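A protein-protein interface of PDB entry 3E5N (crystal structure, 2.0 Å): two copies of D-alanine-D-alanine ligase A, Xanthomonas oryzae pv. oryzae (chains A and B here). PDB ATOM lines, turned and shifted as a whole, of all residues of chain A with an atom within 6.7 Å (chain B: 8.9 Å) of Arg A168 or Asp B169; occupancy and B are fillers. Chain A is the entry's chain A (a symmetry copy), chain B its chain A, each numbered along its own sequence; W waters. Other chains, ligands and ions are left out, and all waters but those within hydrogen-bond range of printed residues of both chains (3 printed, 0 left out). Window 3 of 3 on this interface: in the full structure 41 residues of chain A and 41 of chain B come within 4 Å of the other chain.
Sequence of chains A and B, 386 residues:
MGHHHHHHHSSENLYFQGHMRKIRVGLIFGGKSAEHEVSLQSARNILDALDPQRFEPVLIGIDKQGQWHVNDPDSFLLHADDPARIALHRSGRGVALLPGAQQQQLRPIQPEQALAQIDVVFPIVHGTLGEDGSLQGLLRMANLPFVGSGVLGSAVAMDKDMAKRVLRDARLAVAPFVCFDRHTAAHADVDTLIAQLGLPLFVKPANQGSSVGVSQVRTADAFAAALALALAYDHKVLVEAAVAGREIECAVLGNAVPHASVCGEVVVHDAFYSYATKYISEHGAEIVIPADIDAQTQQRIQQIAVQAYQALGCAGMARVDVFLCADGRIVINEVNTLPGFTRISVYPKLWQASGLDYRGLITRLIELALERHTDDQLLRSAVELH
The side-chain carboxylate (OD1) of Asp A161 is in salt-bridge range of the guanidinium group (NE) of Arg A165 (3.0 Å).
Of chain B, only Asp B169 (2.7 Å) comes within 4 Å of Arg A168. Printed residues of chain A within 4 Å of Asp B169: Arg A165 (3.2 Å) and Arg A168 (2.7 Å). Of the printed residues of chain B, Val A166 touches Met B162 (3.7 Å), Arg B165 (3.5 Å) and Val B166 (3.7 Å). Of the printed residues of chain A, Arg B168 touches Asp A169. Of the printed residues of chain A, Ala B311 touches Met A162 (3.5 Å) and Arg A165 (2.9 Å). Printed residues of chain B within 4 Å of Arg A165: Val B166 (3.5 Å), Asp B169 (3.2 Å) and Ala B311 (2.9 Å). Of the printed residues of chain A, Arg B165 touches Val A166 and Asp A169. Leu A167 touches none of the printed residues of chain B. The nearest residue of chain A that does not touch Asp B169 is Asp A169 (4.2 Å).
The side-chain carboxylate (OD1) of Asp A169 is in salt-bridge range of the guanidinium group (NE) of Arg B168. OD1 of Asp B169 lies within salt-bridge range of NE of Arg A168, at 2.7 Å. The backbone carbonyl oxygen (O) of Ala B311 sits at hydrogen-bond distance from the guanidinium group (NH1) of Arg A165, 2.9 Å away.
Water W3 lies within hydrogen-bond range of OD2 of Asp A169, O of Val A166, NH1 of Arg B165 and N of Ala A170. Water W1 lies within hydrogen-bond range of the side-chain carboxylate of Asp B169 (2.7 Å), the backbone carbonyl oxygen of Val B166 (2.8 Å), the guanidinium group of Arg A165 (2.8 Å) and the backbone NH of Ala B170 (3.4 Å). Water W2 bridges NH2 of Arg A165 (2.9 Å) and O of Ala B311 (3.2 Å).
Of the 16 printed residues of chain B, 7 touch a printed residue of chain A. Hydrophobic or aromatic side chains of chain B that line the printed part of chain A: Met B162 and Val B166. Along chain A the printed residues that touch a printed residue of chain B span positions 162 to 169. Among the printed residues, 12 pairs touch across the chains. Among the printed residues, Asp or Glu carboxylates within 4 Å of a Lys or Arg side-chain nitrogen of the other chain: Arg A168 with Asp B169 and Asp A169 with Arg B168.
Val B166 touches Met A162. CE of Met A162 touches O of Ala B311, 3.5 Å away. Leu B312 touches Met A162 (O to CE, 3.9 Å). Arg A165 touches Val B166 (NH1 to CG1, 3.5 Å). Asp B169 touches Arg A165. Val A166 touches Met B162. CG1 of Val A166 touches NH1 of Arg B165 (3.5 Å). Val A166 touches Val B166. CB of Arg B165 touches OD2 of Asp A169, at 3.2 Å.
Met A162 touches Val B166, and with the chains exchanged Val A166 touches Met B162. Arg A165 touches Val B166, and with the chains exchanged Val A166 touches Arg B165. Arg A165 touches Asp B169, and with the chains exchanged Asp A169 touches Arg B165. Val B166 touches its own counterpart, Val A166. Positions printed for both chains: 162, 163, 164, 165, 166, 167, 168, 169, 170, 171, 172, 173, 174 and 177. Of the 12 pairs that touch across the chains among the printed residues, 9 have their exchanged pair printed and touching as well.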
ATOM      1  N   ASP A 161     -20.567  -0.961  -4.307  1.00  0.00           N
ATOM      2  CA  ASP A 161     -19.413  -1.830  -4.130  1.00  0.00           C
ATOM      3  C   ASP A 161     -18.157  -1.034  -3.869  1.00  0.00           C
ATOM      4  O   ASP A 161     -17.476  -1.206  -2.822  1.00  0.00           O
ATOM      5  CB  ASP A 161     -19.271  -2.791  -5.354  1.00  0.00           C
ATOM      6  CG  ASP A 161     -17.910  -3.461  -5.452  1.00  0.00           C
ATOM      7  OD1 ASP A 161     -17.405  -3.947  -4.418  1.00  0.00           O
ATOM      8  OD2 ASP A 161     -17.361  -3.518  -6.585  1.00  0.00           O
ATOM      9  N   MET A 162     -17.838  -0.137  -4.785  1.00  0.00           N
ATOM     10  CA  MET A 162     -16.583   0.646  -4.667  1.00  0.00           C
ATOM     11  C   MET A 162     -16.636   1.496  -3.370  1.00  0.00           C
ATOM     12  O   MET A 162     -15.673   1.529  -2.565  1.00  0.00           O
ATOM     13  CB  MET A 162     -16.403   1.545  -5.928  1.00  0.00           C
ATOM     14  CG  MET A 162     -15.165   2.374  -5.838  1.00  0.00           C
ATOM     15  SD  MET A 162     -13.678   1.494  -6.132  1.00  0.00           S
ATOM     16  CE  MET A 162     -13.941   0.930  -7.839  1.00  0.00           C
ATOM     17  N   ALA A 163     -17.790   2.102  -3.149  1.00  0.00           N
ATOM     18  CA  ALA A 163     -18.057   2.895  -1.947  1.00  0.00           C
ATOM     19  C   ALA A 163     -17.811   2.148  -0.611  1.00  0.00           C
ATOM     20  O   ALA A 163     -17.109   2.638   0.219  1.00  0.00           O
ATOM     21  CB  ALA A 163     -19.480   3.508  -1.977  1.00  0.00           C
ATOM     22  N   LYS A 164     -18.392   0.962  -0.435  1.00  0.00           N
ATOM     23  CA  LYS A 164     -18.106   0.104   0.731  1.00  0.00           C
ATOM     24  C   LYS A 164     -16.637  -0.284   0.902  1.00  0.00           C
ATOM     25  O   LYS A 164     -16.140  -0.368   2.054  1.00  0.00           O
ATOM     26  CB  LYS A 164     -19.003  -1.150   0.657  1.00  0.00           C
ATOM     27  CG  LYS A 164     -20.494  -0.848   0.902  1.00  0.00           C
ATOM     28  CD  LYS A 164     -21.278  -2.172   0.826  1.00  0.00           C
ATOM     29  CE  LYS A 164     -22.741  -1.904   0.735  1.00  0.00           C
ATOM     30  NZ  LYS A 164     -23.175  -1.246   2.006  1.00  0.00           N
ATOM     31  N   ARG A 165     -15.965  -0.584  -0.219  1.00  0.00           N
ATOM     32  CA  ARG A 165     -14.537  -0.881  -0.217  1.00  0.00           C
ATOM     33  C   ARG A 165     -13.684   0.276   0.240  1.00  0.00           C
ATOM     34  O   ARG A 165     -12.799   0.059   1.075  1.00  0.00           O
ATOM     35  CB  ARG A 165     -14.016  -1.457  -1.506  1.00  0.00           C
ATOM     36  CG  ARG A 165     -14.661  -2.866  -1.869  1.00  0.00           C
ATOM     37  CD  ARG A 165     -13.952  -3.526  -3.074  1.00  0.00           C
ATOM     38  NE  ARG A 165     -14.541  -3.030  -4.297  1.00  0.00           N
ATOM     39  CZ  ARG A 165     -13.893  -2.590  -5.381  1.00  0.00           C
ATOM     40  NH1 ARG A 165     -12.525  -2.542  -5.458  1.00  0.00           N
ATOM     41  NH2 ARG A 165     -14.639  -2.200  -6.417  1.00  0.00           N
ATOM     42  N   VAL A 166     -14.012   1.481  -0.210  1.00  0.00           N
ATOM     43  CA  VAL A 166     -13.301   2.661   0.226  1.00  0.00           C
ATOM     44  C   VAL A 166     -13.539   3.004   1.713  1.00  0.00           C
ATOM     45  O   VAL A 166     -12.588   3.368   2.424  1.00  0.00           O
ATOM     46  CB  VAL A 166     -13.634   3.870  -0.622  1.00  0.00           C
ATOM     47  CG1 VAL A 166     -12.994   5.107   0.016  1.00  0.00           C
ATOM     48  CG2 VAL A 166     -13.036   3.653  -2.034  1.00  0.00           C
ATOM     49  N   LEU A 167     -14.791   2.897   2.158  1.00  0.00           N
ATOM     50  CA  LEU A 167     -15.181   3.103   3.575  1.00  0.00           C
ATOM     51  C   LEU A 167     -14.504   2.051   4.463  1.00  0.00           C
ATOM     52  O   LEU A 167     -14.036   2.368   5.554  1.00  0.00           O
ATOM     53  CB  LEU A 167     -16.718   3.001   3.718  1.00  0.00           C
ATOM     54  CG  LEU A 167     -17.471   4.165   2.996  1.00  0.00           C
ATOM     55  CD1 LEU A 167     -18.957   3.960   3.021  1.00  0.00           C
ATOM     56  CD2 LEU A 167     -17.100   5.558   3.599  1.00  0.00           C
ATOM     57  N   ARG A 168     -14.426   0.810   3.969  1.00  0.00           N
ATOM     58  CA  ARG A 168     -13.843  -0.305   4.722  1.00  0.00           C
ATOM     59  C   ARG A 168     -12.377  -0.020   4.943  1.00  0.00           C
ATOM     60  O   ARG A 168     -11.849  -0.241   6.054  1.00  0.00           O
ATOM     61  CB  ARG A 168     -13.998  -1.623   3.902  1.00  0.00           C
ATOM     62  CG  ARG A 168     -13.169  -2.752   4.352  1.00  0.00           C
ATOM     63  CD  ARG A 168     -13.733  -4.045   3.740  1.00  0.00           C
ATOM     64  NE  ARG A 168     -13.292  -4.233   2.366  1.00  0.00           N
ATOM     65  CZ  ARG A 168     -13.807  -5.128   1.524  1.00  0.00           C
ATOM     66  NH1 ARG A 168     -14.807  -5.921   1.878  1.00  0.00           N
ATOM     67  NH2 ARG A 168     -13.292  -5.258   0.332  1.00  0.00           N
ATOM     68  N   ASP A 169     -11.724   0.442   3.871  1.00  0.00           N
ATOM     69  CA  ASP A 169     -10.313   0.854   3.929  1.00  0.00           C
ATOM     70  C   ASP A 169     -10.108   2.009   4.874  1.00  0.00           C
ATOM     71  O   ASP A 169      -9.078   2.058   5.550  1.00  0.00           O
ATOM     72  CB  ASP A 169      -9.794   1.221   2.539  1.00  0.00           C
ATOM     73  CG  ASP A 169      -8.366   1.703   2.543  1.00  0.00           C
ATOM     74  OD1 ASP A 169      -7.485   0.829   2.670  1.00  0.00           O
ATOM     75  OD2 ASP A 169      -8.145   2.977   2.413  1.00  0.00           O
ATOM     76  N   ALA A 170     -11.063   2.947   4.939  1.00  0.00           N
ATOM     77  CA  ALA A 170     -10.962   4.072   5.903  1.00  0.00           C
ATOM     78  C   ALA A 170     -11.266   3.634   7.349  1.00  0.00           C
ATOM     79  O   ALA A 170     -11.417   4.493   8.194  1.00  0.00           O
ATOM     80  CB  ALA A 170     -11.908   5.215   5.529  1.00  0.00           C
ATOM     81  N   ARG A 171     -11.403   2.331   7.607  1.00  0.00           N
ATOM     82  CA  ARG A 171     -11.666   1.808   8.963  1.00  0.00           C
ATOM     83  C   ARG A 171     -13.043   2.269   9.487  1.00  0.00           C
ATOM     84  O   ARG A 171     -13.240   2.533  10.676  1.00  0.00           O
ATOM     85  CB  ARG A 171     -10.447   2.131   9.897  1.00  0.00           C
ATOM     86  CG  ARG A 171     -10.666   2.123  11.418  1.00  0.00           C
ATOM     87  CD  ARG A 171      -9.556   2.963  12.224  1.00  0.00           C
ATOM     88  NE  ARG A 171      -9.105   2.383  13.522  1.00  0.00           N
ATOM     89  CZ  ARG A 171      -9.634   1.327  14.167  1.00  0.00           C
ATOM     90  NH1 ARG A 171     -10.686   0.647  13.691  1.00  0.00           N
ATOM     91  NH2 ARG A 171      -9.106   0.937  15.322  1.00  0.00           N
ATOM     92  N   LEU A 172     -14.006   2.373   8.571  1.00  0.00           N
ATOM     93  CA  LEU A 172     -15.381   2.625   8.956  1.00  0.00           C
ATOM     94  C   LEU A 172     -16.084   1.308   8.815  1.00  0.00           C
ATOM     95  O   LEU A 172     -15.709   0.479   7.984  1.00  0.00           O
ATOM     96  CB  LEU A 172     -16.024   3.749   8.117  1.00  0.00           C
ATOM     97  CG  LEU A 172     -15.318   5.117   8.218  1.00  0.00           C
ATOM     98  CD1 LEU A 172     -15.674   6.055   7.083  1.00  0.00           C
ATOM     99  CD2 LEU A 172     -15.638   5.810   9.566  1.00  0.00           C
ATOM    100  N   ALA A 173     -17.084   1.097   9.640  1.00  0.00           N
ATOM    101  CA  ALA A 173     -17.806  -0.160   9.643  1.00  0.00           C
ATOM    102  C   ALA A 173     -18.869  -0.147   8.563  1.00  0.00           C
ATOM    103  O   ALA A 173     -19.618   0.819   8.465  1.00  0.00           O
ATOM    104  CB  ALA A 173     -18.449  -0.381  10.976  1.00  0.00           C
ATOM    105  N   VAL A 174     -18.874  -1.185   7.724  1.00  0.00           N
ATOM    106  CA  VAL A 174     -19.939  -1.390   6.727  1.00  0.00           C
ATOM    107  C   VAL A 174     -20.491  -2.804   6.925  1.00  0.00           C
ATOM    108  O   VAL A 174     -19.790  -3.625   7.499  1.00  0.00           O
ATOM    109  CB  VAL A 174     -19.487  -1.076   5.234  1.00  0.00           C
ATOM    110  CG1 VAL A 174     -18.860   0.347   5.097  1.00  0.00           C
ATOM    111  CG2 VAL A 174     -18.490  -2.087   4.706  1.00  0.00           C
ATOM    112  N   PHE A 177     -20.382  -8.053   3.032  1.00  0.00           N
ATOM    113  CA  PHE A 177     -20.952  -8.158   1.692  1.00  0.00           C
ATOM    114  C   PHE A 177     -19.994  -8.860   0.737  1.00  0.00           C
ATOM    115  O   PHE A 177     -18.781  -8.831   0.942  1.00  0.00           O
ATOM    116  CB  PHE A 177     -21.327  -6.770   1.109  1.00  0.00           C
ATOM    117  CG  PHE A 177     -20.165  -6.010   0.625  1.00  0.00           C
ATOM    118  CD1 PHE A 177     -19.883  -5.975  -0.735  1.00  0.00           C
ATOM    119  CD2 PHE A 177     -19.334  -5.341   1.522  1.00  0.00           C
ATOM    120  CE1 PHE A 177     -18.789  -5.246  -1.206  1.00  0.00           C
ATOM    121  CE2 PHE A 177     -18.223  -4.620   1.077  1.00  0.00           C
ATOM    122  CZ  PHE A 177     -17.944  -4.577  -0.314  1.00  0.00           C
ATOM    123  N   MET B 162      -6.836   7.791  -4.030  1.00  0.00           N
ATOM    124  CA  MET B 162      -8.026   6.905  -4.010  1.00  0.00           C
ATOM    125  C   MET B 162      -7.637   5.523  -4.598  1.00  0.00           C
ATOM    126  O   MET B 162      -7.948   4.451  -4.020  1.00  0.00           O
ATOM    127  CB  MET B 162      -9.184   7.561  -4.820  1.00  0.00           C
ATOM    128  CG  MET B 162     -10.394   6.689  -4.851  1.00  0.00           C
ATOM    129  SD  MET B 162     -11.316   6.670  -3.361  1.00  0.00           S
ATOM    130  CE  MET B 162     -11.798   8.416  -3.230  1.00  0.00           C
ATOM    131  N   ALA B 163      -6.895   5.571  -5.691  1.00  0.00           N
ATOM    132  CA  ALA B 163      -6.374   4.375  -6.354  1.00  0.00           C
ATOM    133  C   ALA B 163      -5.556   3.430  -5.438  1.00  0.00           C
ATOM    134  O   ALA B 163      -5.838   2.272  -5.380  1.00  0.00           O
ATOM    135  CB  ALA B 163      -5.566   4.739  -7.626  1.00  0.00           C
ATOM    136  N   LYS B 164      -4.556   3.949  -4.728  1.00  0.00           N
ATOM    137  CA  LYS B 164      -3.814   3.172  -3.716  1.00  0.00           C
ATOM    138  C   LYS B 164      -4.671   2.589  -2.593  1.00  0.00           C
ATOM    139  O   LYS B 164      -4.402   1.455  -2.123  1.00  0.00           O
ATOM    140  CB  LYS B 164      -2.682   4.054  -3.145  1.00  0.00           C
ATOM    141  CG  LYS B 164      -1.554   4.329  -4.158  1.00  0.00           C
ATOM    142  CD  LYS B 164      -0.481   5.192  -3.469  1.00  0.00           C
ATOM    143  CE  LYS B 164       0.463   5.751  -4.479  1.00  0.00           C
ATOM    144  NZ  LYS B 164       1.200   4.613  -5.110  1.00  0.00           N
ATOM    145  N   ARG B 165      -5.649   3.375  -2.119  1.00  0.00           N
ATOM    146  CA  ARG B 165      -6.602   2.916  -1.114  1.00  0.00           C
ATOM    147  C   ARG B 165      -7.459   1.766  -1.581  1.00  0.00           C
ATOM    148  O   ARG B 165      -7.596   0.794  -0.832  1.00  0.00           O
ATOM    149  CB  ARG B 165      -7.445   4.005  -0.509  1.00  0.00           C
ATOM    150  CG  ARG B 165      -6.593   5.086   0.291  1.00  0.00           C
ATOM    151  CD  ARG B 165      -7.501   6.060   1.077  1.00  0.00           C
ATOM    152  NE  ARG B 165      -7.902   7.139   0.204  1.00  0.00           N
ATOM    153  CZ  ARG B 165      -9.136   7.630   0.047  1.00  0.00           C
ATOM    154  NH1 ARG B 165     -10.222   7.135   0.721  1.00  0.00           N
ATOM    155  NH2 ARG B 165      -9.279   8.653  -0.799  1.00  0.00           N
ATOM    156  N   VAL B 166      -7.930   1.830  -2.822  1.00  0.00           N
ATOM    157  CA  VAL B 166      -8.701   0.746  -3.385  1.00  0.00           C
ATOM    158  C   VAL B 166      -7.872  -0.536  -3.622  1.00  0.00           C
ATOM    159  O   VAL B 166      -8.355  -1.645  -3.341  1.00  0.00           O
ATOM    160  CB  VAL B 166      -9.379   1.145  -4.679  1.00  0.00           C
ATOM    161  CG1 VAL B 166     -10.013  -0.101  -5.303  1.00  0.00           C
ATOM    162  CG2 VAL B 166     -10.489   2.174  -4.348  1.00  0.00           C
ATOM    163  N   LEU B 167      -6.656  -0.374  -4.141  1.00  0.00           N
ATOM    164  CA  LEU B 167      -5.695  -1.485  -4.351  1.00  0.00           C
ATOM    165  C   LEU B 167      -5.316  -2.112  -3.004  1.00  0.00           C
ATOM    166  O   LEU B 167      -5.216  -3.331  -2.892  1.00  0.00           O
ATOM    167  CB  LEU B 167      -4.426  -0.958  -5.061  1.00  0.00           C
ATOM    168  CG  LEU B 167      -4.705  -0.481  -6.524  1.00  0.00           C
ATOM    169  CD1 LEU B 167      -3.495   0.165  -7.134  1.00  0.00           C
ATOM    170  CD2 LEU B 167      -5.218  -1.649  -7.426  1.00  0.00           C
ATOM    171  N   ARG B 168      -5.143  -1.271  -1.979  1.00  0.00           N
ATOM    172  CA  ARG B 168      -4.740  -1.724  -0.644  1.00  0.00           C
ATOM    173  C   ARG B 168      -5.835  -2.595  -0.082  1.00  0.00           C
ATOM    174  O   ARG B 168      -5.557  -3.657   0.516  1.00  0.00           O
ATOM    175  CB  ARG B 168      -4.534  -0.485   0.285  1.00  0.00           C
ATOM    176  CG  ARG B 168      -4.469  -0.777   1.725  1.00  0.00           C
ATOM    177  CD  ARG B 168      -3.856   0.439   2.441  1.00  0.00           C
ATOM    178  NE  ARG B 168      -4.839   1.488   2.669  1.00  0.00           N
ATOM    179  CZ  ARG B 168      -4.542   2.730   3.049  1.00  0.00           C
ATOM    180  NH1 ARG B 168      -3.290   3.122   3.228  1.00  0.00           N
ATOM    181  NH2 ARG B 168      -5.508   3.575   3.288  1.00  0.00           N
ATOM    182  N   ASP B 169      -7.077  -2.125  -0.253  1.00  0.00           N
ATOM    183  CA  ASP B 169      -8.268  -2.886   0.154  1.00  0.00           C
ATOM    184  C   ASP B 169      -8.380  -4.187  -0.595  1.00  0.00           C
ATOM    185  O   ASP B 169      -8.815  -5.182  -0.011  1.00  0.00           O
ATOM    186  CB  ASP B 169      -9.537  -2.058  -0.045  1.00  0.00           C
ATOM    187  CG  ASP B 169     -10.798  -2.806   0.306  1.00  0.00           C
ATOM    188  OD1 ASP B 169     -11.045  -2.941   1.520  1.00  0.00           O
ATOM    189  OD2 ASP B 169     -11.538  -3.255  -0.664  1.00  0.00           O
ATOM    190  N   ALA B 170      -8.002  -4.209  -1.881  1.00  0.00           N
ATOM    191  CA  ALA B 170      -8.014  -5.474  -2.658  1.00  0.00           C
ATOM    192  C   ALA B 170      -6.847  -6.406  -2.278  1.00  0.00           C
ATOM    193  O   ALA B 170      -6.629  -7.373  -2.979  1.00  0.00           O
ATOM    194  CB  ALA B 170      -7.955  -5.205  -4.163  1.00  0.00           C
ATOM    195  N   ARG B 171      -6.091  -6.088  -1.225  1.00  0.00           N
ATOM    196  CA  ARG B 171      -4.969  -6.930  -0.763  1.00  0.00           C
ATOM    197  C   ARG B 171      -3.843  -6.995  -1.817  1.00  0.00           C
ATOM    198  O   ARG B 171      -3.171  -8.014  -2.001  1.00  0.00           O
ATOM    199  CB  ARG B 171      -5.519  -8.319  -0.278  1.00  0.00           C
ATOM    200  CG  ARG B 171      -4.546  -9.506  -0.207  1.00  0.00           C
ATOM    201  CD  ARG B 171      -5.287 -10.935  -0.230  1.00  0.00           C
ATOM    202  NE  ARG B 171      -4.709 -11.990   0.651  1.00  0.00           N
ATOM    203  CZ  ARG B 171      -3.551 -11.933   1.335  1.00  0.00           C
ATOM    204  NH1 ARG B 171      -2.744 -10.866   1.294  1.00  0.00           N
ATOM    205  NH2 ARG B 171      -3.182 -12.970   2.080  1.00  0.00           N
ATOM    206  N   LEU B 172      -3.645  -5.881  -2.522  1.00  0.00           N
ATOM    207  CA  LEU B 172      -2.510  -5.752  -3.414  1.00  0.00           C
ATOM    208  C   LEU B 172      -1.535  -4.869  -2.696  1.00  0.00           C
ATOM    209  O   LEU B 172      -1.926  -4.013  -1.900  1.00  0.00           O
ATOM    210  CB  LEU B 172      -2.919  -5.206  -4.800  1.00  0.00           C
ATOM    211  CG  LEU B 172      -3.938  -6.076  -5.563  1.00  0.00           C
ATOM    212  CD1 LEU B 172      -4.642  -5.326  -6.675  1.00  0.00           C
ATOM    213  CD2 LEU B 172      -3.260  -7.337  -6.155  1.00  0.00           C
ATOM    214  N   ALA B 173      -0.264  -5.087  -2.950  1.00  0.00           N
ATOM    215  CA  ALA B 173       0.777  -4.339  -2.274  1.00  0.00           C
ATOM    216  C   ALA B 173       1.000  -3.014  -2.976  1.00  0.00           C
ATOM    217  O   ALA B 173       1.125  -2.991  -4.196  1.00  0.00           O
ATOM    218  CB  ALA B 173       2.052  -5.122  -2.270  1.00  0.00           C
ATOM    219  N   VAL B 174       0.972  -1.924  -2.206  1.00  0.00           N
ATOM    220  CA  VAL B 174       1.324  -0.588  -2.716  1.00  0.00           C
ATOM    221  C   VAL B 174       2.405  -0.013  -1.796  1.00  0.00           C
ATOM    222  O   VAL B 174       2.508  -0.471  -0.666  1.00  0.00           O
ATOM    223  CB  VAL B 174       0.072   0.372  -2.918  1.00  0.00           C
ATOM    224  CG1 VAL B 174      -1.036  -0.286  -3.799  1.00  0.00           C
ATOM    225  CG2 VAL B 174      -0.555   0.792  -1.605  1.00  0.00           C
ATOM    226  N   PHE B 177       2.348   5.151   2.209  1.00  0.00           N
ATOM    227  CA  PHE B 177       2.110   6.543   1.837  1.00  0.00           C
ATOM    228  C   PHE B 177       1.165   7.225   2.819  1.00  0.00           C
ATOM    229  O   PHE B 177       0.352   6.559   3.461  1.00  0.00           O
ATOM    230  CB  PHE B 177       1.531   6.670   0.402  1.00  0.00           C
ATOM    231  CG  PHE B 177       0.102   6.334   0.321  1.00  0.00           C
ATOM    232  CD1 PHE B 177      -0.841   7.353   0.279  1.00  0.00           C
ATOM    233  CD2 PHE B 177      -0.313   5.004   0.304  1.00  0.00           C
ATOM    234  CE1 PHE B 177      -2.201   7.045   0.187  1.00  0.00           C
ATOM    235  CE2 PHE B 177      -1.667   4.672   0.233  1.00  0.00           C
ATOM    236  CZ  PHE B 177      -2.630   5.713   0.179  1.00  0.00           C
ATOM    237  N   ALA B 311      -9.941  -4.311  -9.661  1.00  0.00           N
ATOM    238  CA  ALA B 311     -10.247  -3.565  -8.410  1.00  0.00           C
ATOM    239  C   ALA B 311     -10.650  -2.093  -8.656  1.00  0.00           C
ATOM    240  O   ALA B 311     -11.508  -1.553  -7.981  1.00  0.00           O
ATOM    241  CB  ALA B 311      -9.064  -3.630  -7.409  1.00  0.00           C
ATOM    242  N   LEU B 312      -9.977  -1.442  -9.581  1.00  0.00           N
ATOM    243  CA  LEU B 312     -10.176   0.000  -9.837  1.00  0.00           C
ATOM    244  C   LEU B 312     -11.321   0.229 -10.831  1.00  0.00           C
ATOM    245  O   LEU B 312     -11.722   1.374 -11.054  1.00  0.00           O
ATOM    246  CB  LEU B 312      -8.880   0.597 -10.435  1.00  0.00           C
ATOM    247  CG  LEU B 312      -7.645   0.440  -9.534  1.00  0.00           C
ATOM    248  CD1 LEU B 312      -6.502   1.025 -10.286  1.00  0.00           C
ATOM    249  CD2 LEU B 312      -7.885   1.210  -8.247  1.00  0.00           C
HETATM  250  O   HOH W   1     -10.800  -2.932  -3.284  1.00  0.00           O
HETATM  251  O   HOH W   2     -14.277  -2.524  -9.317  1.00  0.00           O
HETATM  252  O   HOH W   3     -10.213   4.766   2.219  1.00  0.00           O
